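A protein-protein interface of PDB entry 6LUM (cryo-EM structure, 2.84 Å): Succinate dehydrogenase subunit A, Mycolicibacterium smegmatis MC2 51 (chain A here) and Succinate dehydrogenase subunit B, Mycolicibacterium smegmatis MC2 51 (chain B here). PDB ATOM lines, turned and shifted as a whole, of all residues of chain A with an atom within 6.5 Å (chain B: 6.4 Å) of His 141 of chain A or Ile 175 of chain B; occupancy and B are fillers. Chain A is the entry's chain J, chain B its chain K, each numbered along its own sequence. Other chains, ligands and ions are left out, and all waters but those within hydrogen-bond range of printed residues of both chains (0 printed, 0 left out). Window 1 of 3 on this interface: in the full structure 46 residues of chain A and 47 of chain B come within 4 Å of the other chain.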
ATOM      1  N   THR A  40     -29.776 -34.898  12.833  1.00  0.00           N
ATOM      2  CA  THR A  40     -28.840 -33.818  12.573  1.00  0.00           C
ATOM      3  C   THR A  40     -27.386 -34.257  12.643  1.00  0.00           C
ATOM      4  O   THR A  40     -26.495 -33.427  12.475  1.00  0.00           O
ATOM      5  CB  THR A  40     -29.092 -32.673  13.547  1.00  0.00           C
ATOM      6  OG1 THR A  40     -29.350 -33.202  14.850  1.00  0.00           O
ATOM      7  CG2 THR A  40     -30.289 -31.875  13.106  1.00  0.00           C
ATOM      8  N   ARG A  41     -27.124 -35.537  12.876  1.00  0.00           N
ATOM      9  CA  ARG A  41     -25.768 -36.054  12.857  1.00  0.00           C
ATOM     10  C   ARG A  41     -25.422 -36.675  11.521  1.00  0.00           C
ATOM     11  O   ARG A  41     -24.428 -37.394  11.421  1.00  0.00           O
ATOM     12  CB  ARG A  41     -25.574 -37.074  13.974  1.00  0.00           C
ATOM     13  CG  ARG A  41     -25.243 -36.479  15.313  1.00  0.00           C
ATOM     14  CD  ARG A  41     -26.489 -36.033  15.963  1.00  0.00           C
ATOM     15  NE  ARG A  41     -26.349 -35.673  17.359  1.00  0.00           N
ATOM     16  CZ  ARG A  41     -26.200 -34.434  17.789  1.00  0.00           C
ATOM     17  NH1 ARG A  41     -26.137 -33.440  16.932  1.00  0.00           N
ATOM     18  NH2 ARG A  41     -26.110 -34.189  19.077  1.00  0.00           N
ATOM     19  N   THR A  44     -24.853 -35.270   5.530  1.00  0.00           N
ATOM     20  CA  THR A  44     -25.196 -34.045   4.823  1.00  0.00           C
ATOM     21  C   THR A  44     -24.567 -32.844   5.500  1.00  0.00           C
ATOM     22  O   THR A  44     -24.073 -31.934   4.833  1.00  0.00           O
ATOM     23  CB  THR A  44     -26.705 -33.872   4.775  1.00  0.00           C
ATOM     24  OG1 THR A  44     -27.306 -35.096   4.367  1.00  0.00           O
ATOM     25  CG2 THR A  44     -27.083 -32.788   3.817  1.00  0.00           C
ATOM     26  N   GLY A  45     -24.557 -32.840   6.833  1.00  0.00           N
ATOM     27  CA  GLY A  45     -23.984 -31.743   7.579  1.00  0.00           C
ATOM     28  C   GLY A  45     -22.514 -31.522   7.324  1.00  0.00           C
ATOM     29  O   GLY A  45     -21.996 -30.455   7.649  1.00  0.00           O
ATOM     30  N   ALA A  46     -21.822 -32.493   6.749  1.00  0.00           N
ATOM     31  CA  ALA A  46     -20.422 -32.266   6.450  1.00  0.00           C
ATOM     32  C   ALA A  46     -20.223 -31.418   5.212  1.00  0.00           C
ATOM     33  O   ALA A  46     -19.111 -30.936   4.990  1.00  0.00           O
ATOM     34  CB  ALA A  46     -19.689 -33.588   6.274  1.00  0.00           C
ATOM     35  N   ALA A  47     -21.268 -31.218   4.416  1.00  0.00           N
ATOM     36  CA  ALA A  47     -21.165 -30.498   3.155  1.00  0.00           C
ATOM     37  C   ALA A  47     -20.816 -29.042   3.414  1.00  0.00           C
ATOM     38  O   ALA A  47     -21.618 -28.296   3.981  1.00  0.00           O
ATOM     39  CB  ALA A  47     -22.475 -30.614   2.392  1.00  0.00           C
ATOM     40  N   ARG A 138     -20.862 -23.163   5.834  1.00  0.00           N
ATOM     41  CA  ARG A 138     -21.571 -24.333   6.346  1.00  0.00           C
ATOM     42  C   ARG A 138     -22.930 -24.454   5.654  1.00  0.00           C
ATOM     43  O   ARG A 138     -23.954 -24.020   6.165  1.00  0.00           O
ATOM     44  CB  ARG A 138     -21.732 -24.208   7.851  1.00  0.00           C
ATOM     45  CG  ARG A 138     -22.263 -22.846   8.238  1.00  0.00           C
ATOM     46  CD  ARG A 138     -22.140 -22.532   9.687  1.00  0.00           C
ATOM     47  NE  ARG A 138     -22.649 -21.193   9.932  1.00  0.00           N
ATOM     48  CZ  ARG A 138     -21.946 -20.084   9.758  1.00  0.00           C
ATOM     49  NH1 ARG A 138     -20.691 -20.152   9.352  1.00  0.00           N
ATOM     50  NH2 ARG A 138     -22.495 -18.907  10.006  1.00  0.00           N
ATOM     51  N   THR A 139     -22.973 -25.115   4.507  1.00  0.00           N
ATOM     52  CA  THR A 139     -24.236 -25.146   3.780  1.00  0.00           C
ATOM     53  C   THR A 139     -25.057 -26.392   4.088  1.00  0.00           C
ATOM     54  O   THR A 139     -26.271 -26.303   4.302  1.00  0.00           O
ATOM     55  CB  THR A 139     -23.979 -25.055   2.282  1.00  0.00           C
ATOM     56  OG1 THR A 139     -23.036 -24.014   2.029  1.00  0.00           O
ATOM     57  CG2 THR A 139     -25.257 -24.744   1.554  1.00  0.00           C
ATOM     58  N   GLY A 140     -24.416 -27.558   4.090  1.00  0.00           N
ATOM     59  CA  GLY A 140     -25.133 -28.774   4.411  1.00  0.00           C
ATOM     60  C   GLY A 140     -25.702 -28.752   5.808  1.00  0.00           C
ATOM     61  O   GLY A 140     -26.772 -29.302   6.055  1.00  0.00           O
ATOM     62  N   HIS A 141     -25.009 -28.100   6.733  1.00  0.00           N
ATOM     63  CA  HIS A 141     -25.513 -28.003   8.091  1.00  0.00           C
ATOM     64  C   HIS A 141     -26.791 -27.183   8.147  1.00  0.00           C
ATOM     65  O   HIS A 141     -27.720 -27.524   8.882  1.00  0.00           O
ATOM     66  CB  HIS A 141     -24.438 -27.411   8.990  1.00  0.00           C
ATOM     67  CG  HIS A 141     -24.943 -26.990  10.328  1.00  0.00           C
ATOM     68  ND1 HIS A 141     -25.475 -27.879  11.234  1.00  0.00           N
ATOM     69  CD2 HIS A 141     -25.000 -25.771  10.915  1.00  0.00           C
ATOM     70  CE1 HIS A 141     -25.846 -27.224  12.318  1.00  0.00           C
ATOM     71  NE2 HIS A 141     -25.568 -25.944  12.149  1.00  0.00           N
ATOM     72  N   MET A 142     -26.876 -26.115   7.354  1.00  0.00           N
ATOM     73  CA  MET A 142     -28.091 -25.309   7.336  1.00  0.00           C
ATOM     74  C   MET A 142     -29.230 -26.034   6.647  1.00  0.00           C
ATOM     75  O   MET A 142     -30.383 -25.923   7.070  1.00  0.00           O
ATOM     76  CB  MET A 142     -27.838 -23.983   6.642  1.00  0.00           C
ATOM     77  CG  MET A 142     -26.637 -23.254   7.132  1.00  0.00           C
ATOM     78  SD  MET A 142     -26.886 -22.390   8.670  1.00  0.00           S
ATOM     79  CE  MET A 142     -25.594 -21.170   8.501  1.00  0.00           C
ATOM     80  N   ILE A 143     -28.935 -26.767   5.575  1.00  0.00           N
ATOM     81  CA  ILE A 143     -29.967 -27.579   4.934  1.00  0.00           C
ATOM     82  C   ILE A 143     -30.524 -28.596   5.918  1.00  0.00           C
ATOM     83  O   ILE A 143     -31.741 -28.744   6.069  1.00  0.00           O
ATOM     84  CB  ILE A 143     -29.405 -28.271   3.684  1.00  0.00           C
ATOM     85  CG1 ILE A 143     -28.987 -27.249   2.645  1.00  0.00           C
ATOM     86  CG2 ILE A 143     -30.421 -29.204   3.102  1.00  0.00           C
ATOM     87  CD1 ILE A 143     -28.361 -27.867   1.456  1.00  0.00           C
ATOM     88  N   LEU A 144     -29.632 -29.322   6.590  1.00  0.00           N
ATOM     89  CA  LEU A 144     -30.033 -30.319   7.574  1.00  0.00           C
ATOM     90  C   LEU A 144     -30.861 -29.703   8.688  1.00  0.00           C
ATOM     91  O   LEU A 144     -31.903 -30.244   9.070  1.00  0.00           O
ATOM     92  CB  LEU A 144     -28.783 -30.973   8.147  1.00  0.00           C
ATOM     93  CG  LEU A 144     -28.763 -32.421   8.599  1.00  0.00           C
ATOM     94  CD1 LEU A 144     -29.486 -33.270   7.625  1.00  0.00           C
ATOM     95  CD2 LEU A 144     -27.335 -32.845   8.685  1.00  0.00           C
ATOM     96  N   GLN A 145     -30.408 -28.575   9.233  1.00  0.00           N
ATOM     97  CA  GLN A 145     -31.135 -27.939  10.318  1.00  0.00           C
ATOM     98  C   GLN A 145     -32.508 -27.478   9.866  1.00  0.00           C
ATOM     99  O   GLN A 145     -33.485 -27.629  10.597  1.00  0.00           O
ATOM    100  CB  GLN A 145     -30.333 -26.766  10.860  1.00  0.00           C
ATOM    101  CG  GLN A 145     -29.225 -27.162  11.795  1.00  0.00           C
ATOM    102  CD  GLN A 145     -29.629 -27.059  13.241  1.00  0.00           C
ATOM    103  OE1 GLN A 145     -30.700 -27.513  13.627  1.00  0.00           O
ATOM    104  NE2 GLN A 145     -28.779 -26.448  14.053  1.00  0.00           N
ATOM    105  N   THR A 146     -32.607 -26.923   8.660  1.00  0.00           N
ATOM    106  CA  THR A 146     -33.892 -26.448   8.164  1.00  0.00           C
ATOM    107  C   THR A 146     -34.870 -27.593   7.966  1.00  0.00           C
ATOM    108  O   THR A 146     -36.040 -27.499   8.358  1.00  0.00           O
ATOM    109  CB  THR A 146     -33.682 -25.700   6.862  1.00  0.00           C
ATOM    110  OG1 THR A 146     -32.870 -24.555   7.115  1.00  0.00           O
ATOM    111  CG2 THR A 146     -34.990 -25.272   6.298  1.00  0.00           C
ATOM    112  N   VAL B  81     -18.220 -31.470  11.575  1.00  0.00           N
ATOM    113  CA  VAL B  81     -18.702 -31.691  12.934  1.00  0.00           C
ATOM    114  C   VAL B  81     -20.216 -31.715  12.994  1.00  0.00           C
ATOM    115  O   VAL B  81     -20.901 -30.898  12.381  1.00  0.00           O
ATOM    116  CB  VAL B  81     -18.112 -30.640  13.881  1.00  0.00           C
ATOM    117  CG1 VAL B  81     -16.712 -31.062  14.296  1.00  0.00           C
ATOM    118  CG2 VAL B  81     -18.063 -29.327  13.183  1.00  0.00           C
ATOM    119  N   CYS B  82     -20.726 -32.664  13.777  1.00  0.00           N
ATOM    120  CA  CYS B  82     -22.134 -32.990  13.914  1.00  0.00           C
ATOM    121  C   CYS B  82     -22.542 -32.942  15.374  1.00  0.00           C
ATOM    122  O   CYS B  82     -23.712 -32.731  15.693  1.00  0.00           O
ATOM    123  CB  CYS B  82     -22.404 -34.375  13.351  1.00  0.00           C
ATOM    124  SG  CYS B  82     -21.363 -35.652  14.021  1.00  0.00           S
ATOM    125  N   GLY B  83     -21.583 -33.158  16.263  1.00  0.00           N
ATOM    126  CA  GLY B  83     -21.785 -32.916  17.672  1.00  0.00           C
ATOM    127  C   GLY B  83     -22.295 -34.096  18.452  1.00  0.00           C
ATOM    128  O   GLY B  83     -23.107 -33.928  19.356  1.00  0.00           O
ATOM    129  N   SER B  84     -21.828 -35.295  18.136  1.00  0.00           N
ATOM    130  CA  SER B  84     -22.426 -36.472  18.743  1.00  0.00           C
ATOM    131  C   SER B  84     -21.642 -36.965  19.946  1.00  0.00           C
ATOM    132  O   SER B  84     -22.201 -37.656  20.798  1.00  0.00           O
ATOM    133  CB  SER B  84     -22.573 -37.571  17.704  1.00  0.00           C
ATOM    134  OG  SER B  84     -21.329 -37.960  17.196  1.00  0.00           O
ATOM    135  N   LEU B  95     -16.349 -32.592  23.366  1.00  0.00           N
ATOM    136  CA  LEU B  95     -16.335 -33.200  22.024  1.00  0.00           C
ATOM    137  C   LEU B  95     -15.066 -33.974  21.730  1.00  0.00           C
ATOM    138  O   LEU B  95     -14.176 -33.472  21.051  1.00  0.00           O
ATOM    139  CB  LEU B  95     -16.557 -32.195  20.893  1.00  0.00           C
ATOM    140  CG  LEU B  95     -17.838 -32.168  20.080  1.00  0.00           C
ATOM    141  CD1 LEU B  95     -19.050 -31.973  20.893  1.00  0.00           C
ATOM    142  CD2 LEU B  95     -17.686 -31.044  19.128  1.00  0.00           C
ATOM    143  N   THR B 172     -26.504 -19.340  13.986  1.00  0.00           N
ATOM    144  CA  THR B 172     -26.804 -20.357  12.999  1.00  0.00           C
ATOM    145  C   THR B 172     -25.730 -21.424  12.933  1.00  0.00           C
ATOM    146  O   THR B 172     -25.792 -22.293  12.063  1.00  0.00           O
ATOM    147  CB  THR B 172     -26.988 -19.719  11.627  1.00  0.00           C
ATOM    148  OG1 THR B 172     -25.869 -18.883  11.334  1.00  0.00           O
ATOM    149  CG2 THR B 172     -28.239 -18.894  11.601  1.00  0.00           C
ATOM    150  N   LYS B 173     -24.758 -21.386  13.835  1.00  0.00           N
ATOM    151  CA  LYS B 173     -23.661 -22.334  13.858  1.00  0.00           C
ATOM    152  C   LYS B 173     -23.872 -23.471  14.844  1.00  0.00           C
ATOM    153  O   LYS B 173     -22.981 -24.298  15.002  1.00  0.00           O
ATOM    154  CB  LYS B 173     -22.366 -21.619  14.210  1.00  0.00           C
ATOM    155  CG  LYS B 173     -22.084 -20.400  13.413  1.00  0.00           C
ATOM    156  CD  LYS B 173     -20.958 -19.647  14.053  1.00  0.00           C
ATOM    157  CE  LYS B 173     -19.744 -20.526  14.150  1.00  0.00           C
ATOM    158  NZ  LYS B 173     -18.578 -19.810  14.722  1.00  0.00           N
ATOM    159  N   CYS B 174     -25.013 -23.531  15.510  1.00  0.00           N
ATOM    160  CA  CYS B 174     -25.216 -24.493  16.581  1.00  0.00           C
ATOM    161  C   CYS B 174     -25.407 -25.888  16.011  1.00  0.00           C
ATOM    162  O   CYS B 174     -26.347 -26.128  15.253  1.00  0.00           O
ATOM    163  CB  CYS B 174     -26.420 -24.069  17.414  1.00  0.00           C
ATOM    164  SG  CYS B 174     -27.096 -25.268  18.538  1.00  0.00           S
ATOM    165  N   ILE B 175     -24.513 -26.815  16.374  1.00  0.00           N
ATOM    166  CA  ILE B 175     -24.635 -28.202  15.951  1.00  0.00           C
ATOM    167  C   ILE B 175     -25.425 -29.041  16.931  1.00  0.00           C
ATOM    168  O   ILE B 175     -25.573 -30.247  16.714  1.00  0.00           O
ATOM    169  CB  ILE B 175     -23.261 -28.855  15.733  1.00  0.00           C
ATOM    170  CG1 ILE B 175     -22.430 -28.810  16.998  1.00  0.00           C
ATOM    171  CG2 ILE B 175     -22.547 -28.173  14.642  1.00  0.00           C
ATOM    172  CD1 ILE B 175     -21.014 -29.241  16.813  1.00  0.00           C
ATOM    173  N   LEU B 176     -25.939 -28.448  17.998  1.00  0.00           N
ATOM    174  CA  LEU B 176     -26.790 -29.120  18.972  1.00  0.00           C
ATOM    175  C   LEU B 176     -26.076 -30.296  19.625  1.00  0.00           C
ATOM    176  O   LEU B 176     -26.532 -31.431  19.581  1.00  0.00           O
ATOM    177  CB  LEU B 176     -28.096 -29.566  18.327  1.00  0.00           C
ATOM    178  CG  LEU B 176     -29.102 -28.495  17.949  1.00  0.00           C
ATOM    179  CD1 LEU B 176     -30.074 -29.067  16.968  1.00  0.00           C
ATOM    180  CD2 LEU B 176     -29.813 -28.028  19.178  1.00  0.00           C
ATOM    181  N   CYS B 177     -24.952 -30.001  20.266  1.00  0.00           N
ATOM    182  CA  CYS B 177     -24.174 -31.035  20.925  1.00  0.00           C
ATOM    183  C   CYS B 177     -24.421 -31.122  22.422  1.00  0.00           C
ATOM    184  O   CYS B 177     -24.107 -32.155  23.014  1.00  0.00           O
ATOM    185  CB  CYS B 177     -22.682 -30.825  20.668  1.00  0.00           C
ATOM    186  SG  CYS B 177     -21.988 -29.343  21.300  1.00  0.00           S
ATOM    187  N   ALA B 178     -24.976 -30.077  23.031  1.00  0.00           N
ATOM    188  CA  ALA B 178     -25.281 -29.982  24.454  1.00  0.00           C
ATOM    189  C   ALA B 178     -24.053 -29.801  25.322  1.00  0.00           C
ATOM    190  O   ALA B 178     -24.126 -29.992  26.521  1.00  0.00           O
ATOM    191  CB  ALA B 178     -26.078 -31.186  24.946  1.00  0.00           C
ATOM    192  N   PRO B 241     -18.117 -25.677  21.268  1.00  0.00           N
ATOM    193  CA  PRO B 241     -17.054 -26.011  20.321  1.00  0.00           C
ATOM    194  C   PRO B 241     -17.083 -25.234  19.018  1.00  0.00           C
ATOM    195  O   PRO B 241     -16.089 -25.265  18.287  1.00  0.00           O
ATOM    196  CB  PRO B 241     -17.296 -27.493  20.070  1.00  0.00           C
ATOM    197  CG  PRO B 241     -18.684 -27.662  20.284  1.00  0.00           C
ATOM    198  CD  PRO B 241     -19.044 -26.804  21.412  1.00  0.00           C
ATOM    199  N   ARG B 242     -18.172 -24.551  18.693  1.00  0.00           N
ATOM    200  CA  ARG B 242     -18.225 -23.700  17.518  1.00  0.00           C
ATOM    201  C   ARG B 242     -17.859 -22.253  17.812  1.00  0.00           C
ATOM    202  O   ARG B 242     -17.734 -21.466  16.875  1.00  0.00           O
ATOM    203  CB  ARG B 242     -19.617 -23.725  16.896  1.00  0.00           C
ATOM    204  CG  ARG B 242     -20.219 -25.079  16.708  1.00  0.00           C
ATOM    205  CD  ARG B 242     -19.414 -25.938  15.768  1.00  0.00           C
ATOM    206  NE  ARG B 242     -19.024 -25.261  14.540  1.00  0.00           N
ATOM    207  CZ  ARG B 242     -19.798 -25.127  13.471  1.00  0.00           C
ATOM    208  NH1 ARG B 242     -21.022 -25.610  13.463  1.00  0.00           N
ATOM    209  NH2 ARG B 242     -19.345 -24.493  12.406  1.00  0.00           N
ATOM    210  N   ILE B 244     -19.661 -19.693  19.884  1.00  0.00           N
ATOM    211  CA  ILE B 244     -20.886 -19.003  19.509  1.00  0.00           C
ATOM    212  C   ILE B 244     -21.185 -17.760  20.346  1.00  0.00           C
ATOM    213  O   ILE B 244     -21.944 -16.897  19.882  1.00  0.00           O
ATOM    214  CB  ILE B 244     -22.078 -19.985  19.521  1.00  0.00           C
ATOM    215  CG1 ILE B 244     -22.180 -20.692  18.181  1.00  0.00           C
ATOM    216  CG2 ILE B 244     -23.398 -19.321  19.822  1.00  0.00           C
ATOM    217  CD1 ILE B 244     -23.379 -21.521  18.052  1.00  0.00           C
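Among the printed residues, merely in contact across the chains: Arg 138 of chain A with Lys 173 of chain B (3.6 Å), Arg 138 of chain A with Thr 172 of chain B (3.6 Å), His 141 of chain A with Thr 172 of chain B (3.7 Å), Gln 145 of chain A with Leu 176 of chain B (3.7 Å), Arg 41 of chain A with Ser 84 of chain B (3.7 Å) and His 141 of chain A with Ile 175 of chain B (3.95 Å).
The guanidinium group (NH1) of Arg 41 of chain A sits at hydrogen-bond distance from the backbone carbonyl oxygen (O) of Cys 82 of chain B, 2.8 Å away. The guanidinium group of Arg 41 of chain A sits at hydrogen-bond distance from the backbone carbonyl oxygen of Gly 83 of chain B (3.0 Å). The backbone carbonyl oxygen of Ile 175 of chain B is in hydrogen-bond range of the guanidinium group of Arg 41 of chain A, at 3.2 Å. The backbone carbonyl oxygen (O) of Leu 176 of chain B is in hydrogen-bond range of the guanidinium group (NH2) of Arg 41 of chain A, at 2.8 Å. NE2 of His 141 of chain A lies close to O of Cys 174 of chain B (3.2 Å). NE2 of Gln 145 of chain A sits at hydrogen-bond distance from O of Cys 174 of chain B (2.7 Å). O of Thr 172 of chain B lies close to SD of Met 142 of chain A, at 3.6 Å.
O of Met 142 of chain A sits at hydrogen-bond distance from OG1 of Thr 146 of chain A (2.8 Å). NH1 of Arg 242 of chain B is in hydrogen-bond range of O of Lys 173 of chain B (2.8 Å). The side-chain sulfur of Cys 174 of chain B sits close to the backbone NH of Leu 176 of chain B, 3.4 Å away.
His 141 of chain A touches three residues of chain B. Of the printed residues of chain B, Arg 41 of chain A touches Cys 82 (2.8 Å), Gly 83 (3.0 Å), Ser 84 (3.7 Å), Ile 175 (3.2 Å) and Leu 176 (2.8 Å). Of the printed residues of chain A, Cys 174 of chain B touches His 141 and Gln 145. Printed residues of chain A within 4 Å of Gly 83 of chain B: Arg 41 (3.0 Å). Of the printed residues of chain A, Lys 173 of chain B touches Arg 138 (3.6 Å). Ala 47 of chain A touches none of the printed residues of chain B. The nearest residue of chain A that does not touch Ile 175 of chain B is Gln 145 of chain A (4.9 Å).
Of the 15 printed residues of chain A, 5 touch a printed residue of chain B. Hydrophobic or aromatic side chains of chain A that line the printed part of chain B: His 141 and Met 142. Of the 15 printed residues of chain B, 8 touch a printed residue of chain A. Hydrophobic or aromatic side chains of chain B within 4 Å of the printed part of chain A: Leu 176. Among the printed residues, no Asp or Glu carboxylate lies within 4 Å of a Lys or Arg side-chain nitrogen of the other chain.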
